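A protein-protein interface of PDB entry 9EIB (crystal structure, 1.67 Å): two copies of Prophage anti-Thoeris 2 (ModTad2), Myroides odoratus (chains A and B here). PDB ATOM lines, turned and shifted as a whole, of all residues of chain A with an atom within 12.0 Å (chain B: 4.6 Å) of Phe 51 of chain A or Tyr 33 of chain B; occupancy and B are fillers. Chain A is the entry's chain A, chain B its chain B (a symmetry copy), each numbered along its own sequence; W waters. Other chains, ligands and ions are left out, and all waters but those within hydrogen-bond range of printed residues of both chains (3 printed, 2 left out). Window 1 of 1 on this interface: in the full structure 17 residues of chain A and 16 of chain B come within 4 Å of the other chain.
The backbone carbonyl oxygen (O) of Gly 38 of chain A is in hydrogen-bond range of the backbone NH (N) of Tyr 57 of chain A (2.8 Å). O of Tyr 40 of chain A lies within hydrogen-bond range of N of Val 55 of chain A (2.8 Å). The backbone carbonyl oxygen (O) of Val 46 of chain A lies within hydrogen-bond range of the side-chain hydroxyl (OG1) of Thr 50 of chain A. The backbone carbonyl oxygen (O) of Phe 31 of chain B is in hydrogen-bond range of the backbone NH (N) of Lys 64 of chain B (2.9 Å). O of Tyr 33 of chain B sits at hydrogen-bond distance from N of Ala 62 of chain B (2.8 Å). The backbone NH (N) of Val 35 of chain B lies within hydrogen-bond range of the backbone carbonyl oxygen (O) of Tyr 60 of chain B (2.9 Å).
Phe 51 of chain A touches just these residues of chain B: Phe 31, Tyr 33 and Ile 70. Tyr 33 of chain B touches just one residue of chain A: Phe 51. Of chain A, only Thr 50 and Phe 51 come within 4 Å of Phe 31 of chain B. No residue of chain A comes within 4 Å of Ala 32 of chain B. No residue of chain A comes within 4 Å of Val 35 of chain B. Of chain A, only Thr 72 comes within 4 Å of Tyr 60 of chain B. No residue of chain A comes within 4 Å of Leu 61 of chain B. Printed residues of chain B within 4 Å of Val 55 of chain A: Ile 70. Of the printed residues of chain B, Arg 58 of chain A touches Ile 70. Of the printed residues of chain B, Thr 50 of chain A touches Phe 31 and Lys 64. Of the printed residues of chain A, Ile 70 of chain B touches Phe 51, Val 55, Lys 56, Tyr 57 and Arg 58. Printed residues of chain B within 4 Å of Tyr 57 of chain A: Ile 70 (3.4 Å). The nearest residue of chain B that does not touch Phe 51 of chain A is Lys 64 of chain B (4.1 Å).
Of the 12 printed residues of chain B, 5 touch a printed residue of chain A. Printed residues of chain B that touch a printed residue of chain A: Phe 31, Tyr 33, Tyr 60, Lys 64 and Ile 70. Hydrophobic or aromatic side chains of chain A within 4 Å of the printed part of chain B: Phe 51, Val 55 and Tyr 57. Among the printed residues, no Asp or Glu carboxylate lies within 4 Å of a Lys or Arg side-chain nitrogen of the other chain.
1 position is printed for both chains. Of the 10 pairs that touch across the chains among the printed residues, none has its exchanged pair printed and touching as well.
NZ of Lys 64 of chain B lies within hydrogen-bond range of O of Thr 50 of chain A (3.0 Å). The backbone carbonyl oxygen (O) of Lys 56 of chain A is in hydrogen-bond range of the backbone NH (N) of Ile 70 of chain B (3.0 Å). The backbone carbonyl oxygen of Ile 70 of chain B is in hydrogen-bond range of the backbone NH of Arg 58 of chain A, at 2.8 Å.
Water W1 lies within hydrogen-bond range of NZ of Lys 64 of chain B (2.7 Å) and O of Phe 51 of chain A (3.3 Å). Water W3 lies within hydrogen-bond range of the backbone carbonyl oxygen of Arg 58 of chain A (2.7 Å) and the backbone carbonyl oxygen of Ile 70 of chain B (3.1 Å). Water W2 bridges O of Leu 61 of chain B (2.9 Å) and OG1 of Thr 72 of chain A (2.9 Å).
Among the printed residues, merely in contact across the chains: Tyr 57 of chain A with Ile 70 of chain B, Thr 72 of chain A with Tyr 60 of chain B, Phe 51 of chain A with Phe 31 of chain B, Thr 50 of chain A with Phe 31 of chain B, Val 55 of chain A with Ile 70 of chain B, Phe 51 of chain A with Ile 70 of chain B and Phe 51 of chain A with Tyr 33 of chain B.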
ATOM      1  N   GLY A  38       4.008 -14.034 -15.108  1.00  0.00           N
ATOM      2  CA  GLY A  38       2.672 -14.135 -14.553  1.00  0.00           C
ATOM      3  C   GLY A  38       1.602 -14.285 -15.612  1.00  0.00           C
ATOM      4  O   GLY A  38       1.880 -14.607 -16.771  1.00  0.00           O
ATOM      5  N   VAL A  39       0.360 -14.067 -15.172  1.00  0.00           N
ATOM      6  CA  VAL A  39      -0.828 -14.080 -16.017  1.00  0.00           C
ATOM      7  C   VAL A  39      -1.672 -12.854 -15.684  1.00  0.00           C
ATOM      8  O   VAL A  39      -1.793 -12.478 -14.513  1.00  0.00           O
ATOM      9  CB  VAL A  39      -1.648 -15.376 -15.820  1.00  0.00           C
ATOM     10  CG1 VAL A  39      -2.879 -15.382 -16.704  1.00  0.00           C
ATOM     11  CG2 VAL A  39      -0.796 -16.596 -16.105  1.00  0.00           C
ATOM     12  N   TYR A  40      -2.249 -12.224 -16.708  1.00  0.00           N
ATOM     13  CA  TYR A  40      -3.232 -11.166 -16.510  1.00  0.00           C
ATOM     14  C   TYR A  40      -4.368 -11.335 -17.514  1.00  0.00           C
ATOM     15  O   TYR A  40      -4.202 -11.946 -18.577  1.00  0.00           O
ATOM     16  CB  TYR A  40      -2.607  -9.764 -16.626  1.00  0.00           C
ATOM     17  CG  TYR A  40      -2.061  -9.417 -17.995  1.00  0.00           C
ATOM     18  CD1 TYR A  40      -0.748  -9.725 -18.336  1.00  0.00           C
ATOM     19  CD2 TYR A  40      -2.854  -8.766 -18.947  1.00  0.00           C
ATOM     20  CE1 TYR A  40      -0.232  -9.400 -19.586  1.00  0.00           C
ATOM     21  CE2 TYR A  40      -2.351  -8.444 -20.205  1.00  0.00           C
ATOM     22  CZ  TYR A  40      -1.036  -8.760 -20.516  1.00  0.00           C
ATOM     23  OH  TYR A  40      -0.508  -8.442 -21.749  1.00  0.00           O
ATOM     24  N   LYS A  41      -5.531 -10.774 -17.163  1.00  0.00           N
ATOM     25  CA  LYS A  41      -6.747 -10.965 -17.948  1.00  0.00           C
ATOM     26  C   LYS A  41      -6.821  -9.989 -19.115  1.00  0.00           C
ATOM     27  O   LYS A  41      -6.502  -8.805 -18.975  1.00  0.00           O
ATOM     28  CB  LYS A  41      -7.983 -10.789 -17.066  1.00  0.00           C
ATOM     29  CG  LYS A  41      -8.028 -11.696 -15.851  1.00  0.00           C
ATOM     30  CD  LYS A  41      -9.213 -11.352 -14.966  1.00  0.00           C
ATOM     31  CE  LYS A  41     -10.520 -11.552 -15.708  1.00  0.00           C
ATOM     32  NZ  LYS A  41     -10.644 -12.953 -16.185  1.00  0.00           N
ATOM     33  N   SER A  42      -7.248 -10.494 -20.273  1.00  0.00           N
ATOM     34  CA  SER A  42      -7.550  -9.620 -21.401  1.00  0.00           C
ATOM     35  C   SER A  42      -8.788  -8.797 -21.074  1.00  0.00           C
ATOM     36  O   SER A  42      -9.828  -9.348 -20.698  1.00  0.00           O
ATOM     37  CB  SER A  42      -7.777 -10.433 -22.678  1.00  0.00           C
ATOM     38  OG  SER A  42      -6.554 -10.784 -23.308  1.00  0.00           O
ATOM     39  N   GLN A  43      -8.678  -7.474 -21.209  1.00  0.00           N
ATOM     40  CA  GLN A  43      -9.741  -6.602 -20.732  1.00  0.00           C
ATOM     41  C   GLN A  43     -10.678  -6.113 -21.828  1.00  0.00           C
ATOM     42  O   GLN A  43     -11.825  -5.767 -21.527  1.00  0.00           O
ATOM     43  CB  GLN A  43      -9.149  -5.404 -19.982  1.00  0.00           C
ATOM     44  CG  GLN A  43      -8.643  -5.766 -18.586  1.00  0.00           C
ATOM     45  CD  GLN A  43      -9.700  -6.468 -17.732  1.00  0.00           C
ATOM     46  OE1 GLN A  43     -10.878  -6.109 -17.758  1.00  0.00           O
ATOM     47  NE2 GLN A  43      -9.278  -7.479 -16.977  1.00  0.00           N
ATOM     48  N   THR A  44     -10.236  -6.090 -23.078  1.00  0.00           N
ATOM     49  CA  THR A  44     -11.105  -5.743 -24.190  1.00  0.00           C
ATOM     50  C   THR A  44     -11.168  -6.905 -25.170  1.00  0.00           C
ATOM     51  O   THR A  44     -10.245  -7.722 -25.254  1.00  0.00           O
ATOM     52  CB  THR A  44     -10.621  -4.482 -24.919  1.00  0.00           C
ATOM     53  OG1 THR A  44      -9.347  -4.739 -25.517  1.00  0.00           O
ATOM     54  CG2 THR A  44     -10.502  -3.305 -23.956  1.00  0.00           C
ATOM     55  N   ASP A  45     -12.275  -6.973 -25.916  1.00  0.00           N
ATOM     56  CA  ASP A  45     -12.398  -7.994 -26.951  1.00  0.00           C
ATOM     57  C   ASP A  45     -11.337  -7.822 -28.029  1.00  0.00           C
ATOM     58  O   ASP A  45     -10.967  -8.797 -28.691  1.00  0.00           O
ATOM     59  CB  ASP A  45     -13.792  -7.961 -27.578  1.00  0.00           C
ATOM     60  CG  ASP A  45     -14.893  -8.081 -26.553  1.00  0.00           C
ATOM     61  OD1 ASP A  45     -14.628  -8.601 -25.444  1.00  0.00           O
ATOM     62  OD2 ASP A  45     -16.025  -7.649 -26.857  1.00  0.00           O
ATOM     63  N   VAL A  46     -10.848  -6.595 -28.233  1.00  0.00           N
ATOM     64  CA  VAL A  46      -9.736  -6.394 -29.159  1.00  0.00           C
ATOM     65  C   VAL A  46      -8.495  -7.114 -28.648  1.00  0.00           C
ATOM     66  O   VAL A  46      -7.814  -7.829 -29.396  1.00  0.00           O
ATOM     67  CB  VAL A  46      -9.462  -4.895 -29.372  1.00  0.00           C
ATOM     68  CG1 VAL A  46      -8.293  -4.720 -30.334  1.00  0.00           C
ATOM     69  CG2 VAL A  46     -10.708  -4.178 -29.890  1.00  0.00           C
ATOM     70  N   ILE A  47      -8.187  -6.935 -27.359  1.00  0.00           N
ATOM     71  CA  ILE A  47      -7.088  -7.667 -26.739  1.00  0.00           C
ATOM     72  C   ILE A  47      -7.423  -9.149 -26.641  1.00  0.00           C
ATOM     73  O   ILE A  47      -6.566 -10.011 -26.868  1.00  0.00           O
ATOM     74  CB  ILE A  47      -6.766  -7.063 -25.360  1.00  0.00           C
ATOM     75  CG1 ILE A  47      -6.333  -5.598 -25.512  1.00  0.00           C
ATOM     76  CG2 ILE A  47      -5.700  -7.898 -24.652  1.00  0.00           C
ATOM     77  CD1 ILE A  47      -6.349  -4.794 -24.215  1.00  0.00           C
ATOM     78  N   LYS A  48      -8.679  -9.468 -26.312  1.00  0.00           N
ATOM     79  CA  LYS A  48      -9.101 -10.862 -26.210  1.00  0.00           C
ATOM     80  C   LYS A  48      -8.898 -11.605 -27.526  1.00  0.00           C
ATOM     81  O   LYS A  48      -8.514 -12.779 -27.532  1.00  0.00           O
ATOM     82  CB  LYS A  48     -10.564 -10.923 -25.767  1.00  0.00           C
ATOM     83  CG  LYS A  48     -11.153 -12.318 -25.681  1.00  0.00           C
ATOM     84  CD  LYS A  48     -12.586 -12.264 -25.156  1.00  0.00           C
ATOM     85  CE  LYS A  48     -13.286 -13.610 -25.301  1.00  0.00           C
ATOM     86  NZ  LYS A  48     -12.558 -14.684 -24.579  1.00  0.00           N
ATOM     87  N   ASN A  49      -9.143 -10.939 -28.654  1.00  0.00           N
ATOM     88  CA  ASN A  49      -8.931 -11.586 -29.946  1.00  0.00           C
ATOM     89  C   ASN A  49      -7.446 -11.773 -30.235  1.00  0.00           C
ATOM     90  O   ASN A  49      -7.029 -12.841 -30.701  1.00  0.00           O
ATOM     91  CB  ASN A  49      -9.597 -10.776 -31.063  1.00  0.00           C
ATOM     92  CG  ASN A  49     -11.113 -10.939 -31.088  1.00  0.00           C
ATOM     93  OD1 ASN A  49     -11.640 -11.999 -30.749  1.00  0.00           O
ATOM     94  ND2 ASN A  49     -11.818  -9.887 -31.495  1.00  0.00           N
ATOM     95  N   THR A  50      -6.632 -10.750 -29.953  1.00  0.00           N
ATOM     96  CA  THR A  50      -5.213 -10.813 -30.297  1.00  0.00           C
ATOM     97  C   THR A  50      -4.475 -11.845 -29.443  1.00  0.00           C
ATOM     98  O   THR A  50      -3.695 -12.649 -29.966  1.00  0.00           O
ATOM     99  CB  THR A  50      -4.560  -9.428 -30.159  1.00  0.00           C
ATOM    100  OG1 THR A  50      -5.313  -8.448 -30.884  1.00  0.00           O
ATOM    101  CG2 THR A  50      -3.154  -9.444 -30.728  1.00  0.00           C
ATOM    102  N   PHE A  51      -4.719 -11.853 -28.128  1.00  0.00           N
ATOM    103  CA  PHE A  51      -3.920 -12.649 -27.198  1.00  0.00           C
ATOM    104  C   PHE A  51      -4.703 -13.735 -26.473  1.00  0.00           C
ATOM    105  O   PHE A  51      -4.136 -14.392 -25.593  1.00  0.00           O
ATOM    106  CB  PHE A  51      -3.263 -11.757 -26.143  1.00  0.00           C
ATOM    107  CG  PHE A  51      -2.455 -10.627 -26.704  1.00  0.00           C
ATOM    108  CD1 PHE A  51      -3.032  -9.372 -26.895  1.00  0.00           C
ATOM    109  CD2 PHE A  51      -1.115 -10.800 -27.008  1.00  0.00           C
ATOM    110  CE1 PHE A  51      -2.292  -8.306 -27.403  1.00  0.00           C
ATOM    111  CE2 PHE A  51      -0.364  -9.742 -27.515  1.00  0.00           C
ATOM    112  CZ  PHE A  51      -0.959  -8.487 -27.709  1.00  0.00           C
ATOM    113  N   GLY A  52      -5.980 -13.934 -26.788  1.00  0.00           N
ATOM    114  CA  GLY A  52      -6.795 -14.857 -26.013  1.00  0.00           C
ATOM    115  C   GLY A  52      -7.376 -14.200 -24.772  1.00  0.00           C
ATOM    116  O   GLY A  52      -7.220 -12.999 -24.534  1.00  0.00           O
ATOM    117  N   GLU A  53      -8.048 -15.019 -23.954  1.00  0.00           N
ATOM    118  CA  GLU A  53      -8.786 -14.478 -22.814  1.00  0.00           C
ATOM    119  C   GLU A  53      -7.866 -14.077 -21.663  1.00  0.00           C
ATOM    120  O   GLU A  53      -8.124 -13.072 -20.985  1.00  0.00           O
ATOM    121  CB  GLU A  53      -9.837 -15.485 -22.334  1.00  0.00           C
ATOM    122  CG  GLU A  53     -10.838 -14.897 -21.341  1.00  0.00           C
ATOM    123  CD  GLU A  53     -12.232 -15.503 -21.462  1.00  0.00           C
ATOM    124  OE1 GLU A  53     -12.403 -16.452 -22.256  1.00  0.00           O
ATOM    125  OE2 GLU A  53     -13.157 -15.022 -20.768  1.00  0.00           O
ATOM    126  N   GLU A  54      -6.808 -14.848 -21.408  1.00  0.00           N
ATOM    127  CA  GLU A  54      -5.804 -14.492 -20.414  1.00  0.00           C
ATOM    128  C   GLU A  54      -4.412 -14.703 -20.984  1.00  0.00           C
ATOM    129  O   GLU A  54      -4.176 -15.621 -21.777  1.00  0.00           O
ATOM    130  CB  GLU A  54      -5.953 -15.286 -19.129  1.00  0.00           C
ATOM    131  CG  GLU A  54      -7.005 -14.698 -18.212  1.00  0.00           C
ATOM    132  CD  GLU A  54      -7.014 -15.349 -16.853  1.00  0.00           C
ATOM    133  OE1 GLU A  54      -6.153 -16.225 -16.616  1.00  0.00           O
ATOM    134  OE2 GLU A  54      -7.881 -14.981 -16.027  1.00  0.00           O
ATOM    135  N   VAL A  55      -3.490 -13.844 -20.563  1.00  0.00           N
ATOM    136  CA  VAL A  55      -2.190 -13.702 -21.208  1.00  0.00           C
ATOM    137  C   VAL A  55      -1.094 -14.061 -20.215  1.00  0.00           C
ATOM    138  O   VAL A  55      -1.001 -13.457 -19.138  1.00  0.00           O
ATOM    139  CB  VAL A  55      -1.982 -12.279 -21.744  1.00  0.00           C
ATOM    140  CG1 VAL A  55      -1.080 -12.320 -22.964  1.00  0.00           C
ATOM    141  CG2 VAL A  55      -3.319 -11.629 -22.057  1.00  0.00           C
ATOM    142  N   LYS A  56      -0.253 -15.017 -20.594  1.00  0.00           N
ATOM    143  CA  LYS A  56       0.936 -15.354 -19.824  1.00  0.00           C
ATOM    144  C   LYS A  56       2.107 -14.488 -20.279  1.00  0.00           C
ATOM    145  O   LYS A  56       2.333 -14.333 -21.486  1.00  0.00           O
ATOM    146  CB  LYS A  56       1.270 -16.828 -20.008  1.00  0.00           C
ATOM    147  CG  LYS A  56       2.074 -17.436 -18.885  1.00  0.00           C
ATOM    148  CD  LYS A  56       2.112 -18.957 -19.007  1.00  0.00           C
ATOM    149  CE  LYS A  56       2.937 -19.396 -20.209  1.00  0.00           C
ATOM    150  NZ  LYS A  56       3.067 -20.879 -20.296  1.00  0.00           N
ATOM    151  N   TYR A  57       2.853 -13.925 -19.328  1.00  0.00           N
ATOM    152  CA  TYR A  57       4.053 -13.167 -19.672  1.00  0.00           C
ATOM    153  C   TYR A  57       5.271 -13.757 -18.970  1.00  0.00           C
ATOM    154  O   TYR A  57       5.193 -14.168 -17.811  1.00  0.00           O
ATOM    155  CB  TYR A  57       3.898 -11.683 -19.350  1.00  0.00           C
ATOM    156  CG  TYR A  57       3.692 -11.347 -17.909  1.00  0.00           C
ATOM    157  CD1 TYR A  57       4.778 -11.165 -17.065  1.00  0.00           C
ATOM    158  CD2 TYR A  57       2.403 -11.174 -17.390  1.00  0.00           C
ATOM    159  CE1 TYR A  57       4.590 -10.842 -15.714  1.00  0.00           C
ATOM    160  CE2 TYR A  57       2.203 -10.859 -16.043  1.00  0.00           C
ATOM    161  CZ  TYR A  57       3.306 -10.694 -15.211  1.00  0.00           C
ATOM    162  OH  TYR A  57       3.131 -10.381 -13.876  1.00  0.00           O
ATOM    163  N   ARG A  58       6.391 -13.800 -19.688  1.00  0.00           N
ATOM    164  CA  ARG A  58       7.594 -14.435 -19.181  1.00  0.00           C
ATOM    165  C   ARG A  58       8.278 -13.567 -18.131  1.00  0.00           C
ATOM    166  O   ARG A  58       8.068 -12.353 -18.083  1.00  0.00           O
ATOM    167  CB  ARG A  58       8.563 -14.697 -20.324  1.00  0.00           C
ATOM    168  CG  ARG A  58       8.084 -15.704 -21.317  1.00  0.00           C
ATOM    169  CD  ARG A  58       9.263 -16.169 -22.106  1.00  0.00           C
ATOM    170  NE  ARG A  58       8.871 -16.851 -23.326  1.00  0.00           N
ATOM    171  CZ  ARG A  58       9.728 -17.445 -24.135  1.00  0.00           C
ATOM    172  NH1 ARG A  58      11.024 -17.465 -23.867  1.00  0.00           N
ATOM    173  NH2 ARG A  58       9.277 -18.035 -25.239  1.00  0.00           N
ATOM    174  N   TYR A  60      11.476 -11.491 -16.624  1.00  0.00           N
ATOM    175  CA  TYR A  60      12.390 -10.606 -17.341  1.00  0.00           C
ATOM    176  C   TYR A  60      13.350  -9.994 -16.325  1.00  0.00           C
ATOM    177  O   TYR A  60      13.277 -10.284 -15.130  1.00  0.00           O
ATOM    178  CB  TYR A  60      11.607  -9.550 -18.149  1.00  0.00           C
ATOM    179  CG  TYR A  60      10.757  -8.638 -17.302  1.00  0.00           C
ATOM    180  CD1 TYR A  60       9.478  -9.023 -16.880  1.00  0.00           C
ATOM    181  CD2 TYR A  60      11.225  -7.389 -16.913  1.00  0.00           C
ATOM    182  CE1 TYR A  60       8.691  -8.174 -16.094  1.00  0.00           C
ATOM    183  CE2 TYR A  60      10.450  -6.540 -16.140  1.00  0.00           C
ATOM    184  CZ  TYR A  60       9.190  -6.938 -15.731  1.00  0.00           C
ATOM    185  OH  TYR A  60       8.443  -6.081 -14.959  1.00  0.00           O
ATOM    186  N   THR A  72      13.578  -2.079 -18.942  1.00  0.00           N
ATOM    187  CA  THR A  72      13.820  -3.490 -19.200  1.00  0.00           C
ATOM    188  C   THR A  72      15.261  -3.647 -19.654  1.00  0.00           C
ATOM    189  O   THR A  72      15.805  -2.803 -20.367  1.00  0.00           O
ATOM    190  CB  THR A  72      12.867  -4.050 -20.260  1.00  0.00           C
ATOM    191  OG1 THR A  72      13.086  -3.384 -21.509  1.00  0.00           O
ATOM    192  CG2 THR A  72      11.433  -3.876 -19.832  1.00  0.00           C
ATOM    193  N   LEU B  14       5.951   0.822 -34.616  1.00  0.00           N
ATOM    194  CA  LEU B  14       5.887   0.436 -33.208  1.00  0.00           C
ATOM    195  C   LEU B  14       5.440   1.607 -32.349  1.00  0.00           C
ATOM    196  O   LEU B  14       4.522   1.476 -31.525  1.00  0.00           O
ATOM    197  CB  LEU B  14       7.248  -0.079 -32.759  1.00  0.00           C
ATOM    198  CG  LEU B  14       7.584  -1.513 -33.175  1.00  0.00           C
ATOM    199  CD1 LEU B  14       9.100  -1.778 -33.052  1.00  0.00           C
ATOM    200  CD2 LEU B  14       6.784  -2.467 -32.296  1.00  0.00           C
ATOM    201  N   LYS B  18       1.391   0.000 -33.617  1.00  0.00           N
ATOM    202  CA  LYS B  18       1.145  -1.130 -34.501  1.00  0.00           C
ATOM    203  C   LYS B  18       1.996  -2.333 -34.123  1.00  0.00           C
ATOM    204  O   LYS B  18       2.995  -2.213 -33.411  1.00  0.00           O
ATOM    205  CB  LYS B  18       1.434  -0.727 -35.944  1.00  0.00           C
ATOM    206  CG  LYS B  18       0.594   0.438 -36.428  1.00  0.00           C
ATOM    207  CD  LYS B  18       0.945   0.767 -37.862  1.00  0.00           C
ATOM    208  CE  LYS B  18      -0.001   1.830 -38.413  1.00  0.00           C
ATOM    209  NZ  LYS B  18       0.470   2.296 -39.740  1.00  0.00           N
ATOM    210  N   PHE B  31       4.943 -11.382 -33.306  1.00  0.00           N
ATOM    211  CA  PHE B  31       4.962  -9.956 -33.603  1.00  0.00           C
ATOM    212  C   PHE B  31       5.452  -9.200 -32.373  1.00  0.00           C
ATOM    213  O   PHE B  31       5.254  -9.645 -31.234  1.00  0.00           O
ATOM    214  CB  PHE B  31       3.582  -9.429 -34.046  1.00  0.00           C
ATOM    215  CG  PHE B  31       2.502  -9.603 -33.006  1.00  0.00           C
ATOM    216  CD1 PHE B  31       2.350  -8.688 -31.974  1.00  0.00           C
ATOM    217  CD2 PHE B  31       1.636 -10.677 -33.067  1.00  0.00           C
ATOM    218  CE1 PHE B  31       1.377  -8.858 -31.010  1.00  0.00           C
ATOM    219  CE2 PHE B  31       0.632 -10.842 -32.106  1.00  0.00           C
ATOM    220  CZ  PHE B  31       0.502  -9.943 -31.084  1.00  0.00           C
ATOM    221  N   ALA B  32       6.066  -8.043 -32.615  1.00  0.00           N
ATOM    222  CA  ALA B  32       6.489  -7.144 -31.555  1.00  0.00           C
ATOM    223  C   ALA B  32       5.576  -5.918 -31.480  1.00  0.00           C
ATOM    224  O   ALA B  32       4.936  -5.532 -32.464  1.00  0.00           O
ATOM    225  CB  ALA B  32       7.952  -6.733 -31.761  1.00  0.00           C
ATOM    226  N   TYR B  33       5.507  -5.314 -30.290  1.00  0.00           N
ATOM    227  CA  TYR B  33       4.687  -4.132 -30.060  1.00  0.00           C
ATOM    228  C   TYR B  33       5.272  -3.311 -28.915  1.00  0.00           C
ATOM    229  O   TYR B  33       6.078  -3.792 -28.106  1.00  0.00           O
ATOM    230  CB  TYR B  33       3.218  -4.487 -29.782  1.00  0.00           C
ATOM    231  CG  TYR B  33       2.973  -5.315 -28.542  1.00  0.00           C
ATOM    232  CD1 TYR B  33       3.126  -6.691 -28.569  1.00  0.00           C
ATOM    233  CD2 TYR B  33       2.565  -4.727 -27.349  1.00  0.00           C
ATOM    234  CE1 TYR B  33       2.893  -7.471 -27.446  1.00  0.00           C
ATOM    235  CE2 TYR B  33       2.336  -5.507 -26.215  1.00  0.00           C
ATOM    236  CZ  TYR B  33       2.493  -6.878 -26.282  1.00  0.00           C
ATOM    237  OH  TYR B  33       2.270  -7.690 -25.178  1.00  0.00           O
ATOM    238  N   TYR B  34       4.849  -2.058 -28.873  1.00  0.00           N
ATOM    239  CA  TYR B  34       5.313  -1.055 -27.923  1.00  0.00           C
ATOM    240  C   TYR B  34       4.404  -1.002 -26.705  1.00  0.00           C
ATOM    241  O   TYR B  34       3.177  -1.090 -26.828  1.00  0.00           O
ATOM    242  CB  TYR B  34       5.307   0.302 -28.627  1.00  0.00           C
ATOM    243  CG  TYR B  34       5.688   1.530 -27.831  1.00  0.00           C
ATOM    244  CD1 TYR B  34       4.745   2.228 -27.081  1.00  0.00           C
ATOM    245  CD2 TYR B  34       6.983   2.021 -27.867  1.00  0.00           C
ATOM    246  CE1 TYR B  34       5.096   3.375 -26.378  1.00  0.00           C
ATOM    247  CE2 TYR B  34       7.336   3.181 -27.173  1.00  0.00           C
ATOM    248  CZ  TYR B  34       6.394   3.831 -26.425  1.00  0.00           C
ATOM    249  OH  TYR B  34       6.750   4.972 -25.744  1.00  0.00           O
ATOM    250  N   VAL B  35       5.001  -0.812 -25.530  1.00  0.00           N
ATOM    251  CA  VAL B  35       4.263  -0.643 -24.286  1.00  0.00           C
ATOM    252  C   VAL B  35       4.700   0.674 -23.654  1.00  0.00           C
ATOM    253  O   VAL B  35       5.896   0.883 -23.438  1.00  0.00           O
ATOM    254  CB  VAL B  35       4.481  -1.808 -23.309  1.00  0.00           C
ATOM    255  CG1 VAL B  35       3.564  -1.632 -22.100  1.00  0.00           C
ATOM    256  CG2 VAL B  35       4.203  -3.131 -23.997  1.00  0.00           C
ATOM    257  N   TYR B  60       8.756   0.203 -23.128  1.00  0.00           N
ATOM    258  CA  TYR B  60       9.578  -0.925 -23.549  1.00  0.00           C
ATOM    259  C   TYR B  60       8.905  -1.618 -24.725  1.00  0.00           C
ATOM    260  O   TYR B  60       7.834  -1.208 -25.183  1.00  0.00           O
ATOM    261  CB  TYR B  60       9.824  -1.885 -22.382  1.00  0.00           C
ATOM    262  CG  TYR B  60       8.564  -2.508 -21.833  1.00  0.00           C
ATOM    263  CD1 TYR B  60       7.796  -1.843 -20.891  1.00  0.00           C
ATOM    264  CD2 TYR B  60       8.160  -3.773 -22.251  1.00  0.00           C
ATOM    265  CE1 TYR B  60       6.638  -2.412 -20.363  1.00  0.00           C
ATOM    266  CE2 TYR B  60       7.010  -4.349 -21.735  1.00  0.00           C
ATOM    267  CZ  TYR B  60       6.259  -3.661 -20.794  1.00  0.00           C
ATOM    268  OH  TYR B  60       5.127  -4.231 -20.288  1.00  0.00           O
ATOM    269  N   LEU B  61       9.560  -2.645 -25.245  1.00  0.00           N
ATOM    270  CA  LEU B  61       9.038  -3.412 -26.362  1.00  0.00           C
ATOM    271  C   LEU B  61       8.737  -4.836 -25.911  1.00  0.00           C
ATOM    272  O   LEU B  61       9.439  -5.396 -25.060  1.00  0.00           O
ATOM    273  CB  LEU B  61      10.032  -3.404 -27.528  1.00  0.00           C
ATOM    274  CG  LEU B  61      10.394  -2.016 -28.078  1.00  0.00           C
ATOM    275  CD1 LEU B  61      11.409  -2.165 -29.222  1.00  0.00           C
ATOM    276  CD2 LEU B  61       9.184  -1.282 -28.584  1.00  0.00           C
ATOM    277  N   ALA B  62       7.686  -5.429 -26.488  1.00  0.00           N
ATOM    278  CA  ALA B  62       7.260  -6.777 -26.129  1.00  0.00           C
ATOM    279  C   ALA B  62       7.146  -7.636 -27.378  1.00  0.00           C
ATOM    280  O   ALA B  62       6.916  -7.133 -28.479  1.00  0.00           O
ATOM    281  CB  ALA B  62       5.927  -6.763 -25.401  1.00  0.00           C
ATOM    282  N   LYS B  64       5.180 -11.177 -28.794  1.00  0.00           N
ATOM    283  CA  LYS B  64       4.323 -12.361 -28.698  1.00  0.00           C
ATOM    284  C   LYS B  64       5.054 -13.530 -29.358  1.00  0.00           C
ATOM    285  O   LYS B  64       5.223 -13.554 -30.583  1.00  0.00           O
ATOM    286  CB  LYS B  64       2.968 -12.113 -29.358  1.00  0.00           C
ATOM    287  CG  LYS B  64       2.332 -13.407 -29.902  1.00  0.00           C
ATOM    288  CD  LYS B  64       0.983 -13.625 -29.334  1.00  0.00           C
ATOM    289  CE  LYS B  64       0.107 -14.446 -30.290  1.00  0.00           C
ATOM    290  NZ  LYS B  64      -1.344 -14.509 -29.841  1.00  0.00           N
ATOM    291  N   ILE B  70       4.221 -13.693 -23.668  1.00  0.00           N
ATOM    292  CA  ILE B  70       4.783 -12.378 -23.960  1.00  0.00           C
ATOM    293  C   ILE B  70       6.148 -12.271 -23.305  1.00  0.00           C
ATOM    294  O   ILE B  70       6.285 -12.443 -22.083  1.00  0.00           O
ATOM    295  CB  ILE B  70       3.869 -11.249 -23.474  1.00  0.00           C
ATOM    296  CG1 ILE B  70       2.459 -11.455 -24.014  1.00  0.00           C
ATOM    297  CG2 ILE B  70       4.440  -9.896 -23.901  1.00  0.00           C
ATOM    298  CD1 ILE B  70       2.395 -11.495 -25.524  1.00  0.00           C
HETATM  299  O   HOH W   1      -1.254 -14.442 -27.155  1.00  0.00           O
HETATM  300  O   HOH W   2      11.830  -4.085 -24.083  1.00  0.00           O
HETATM  301  O   HOH W   3       7.744 -10.577 -20.132  1.00  0.00           O
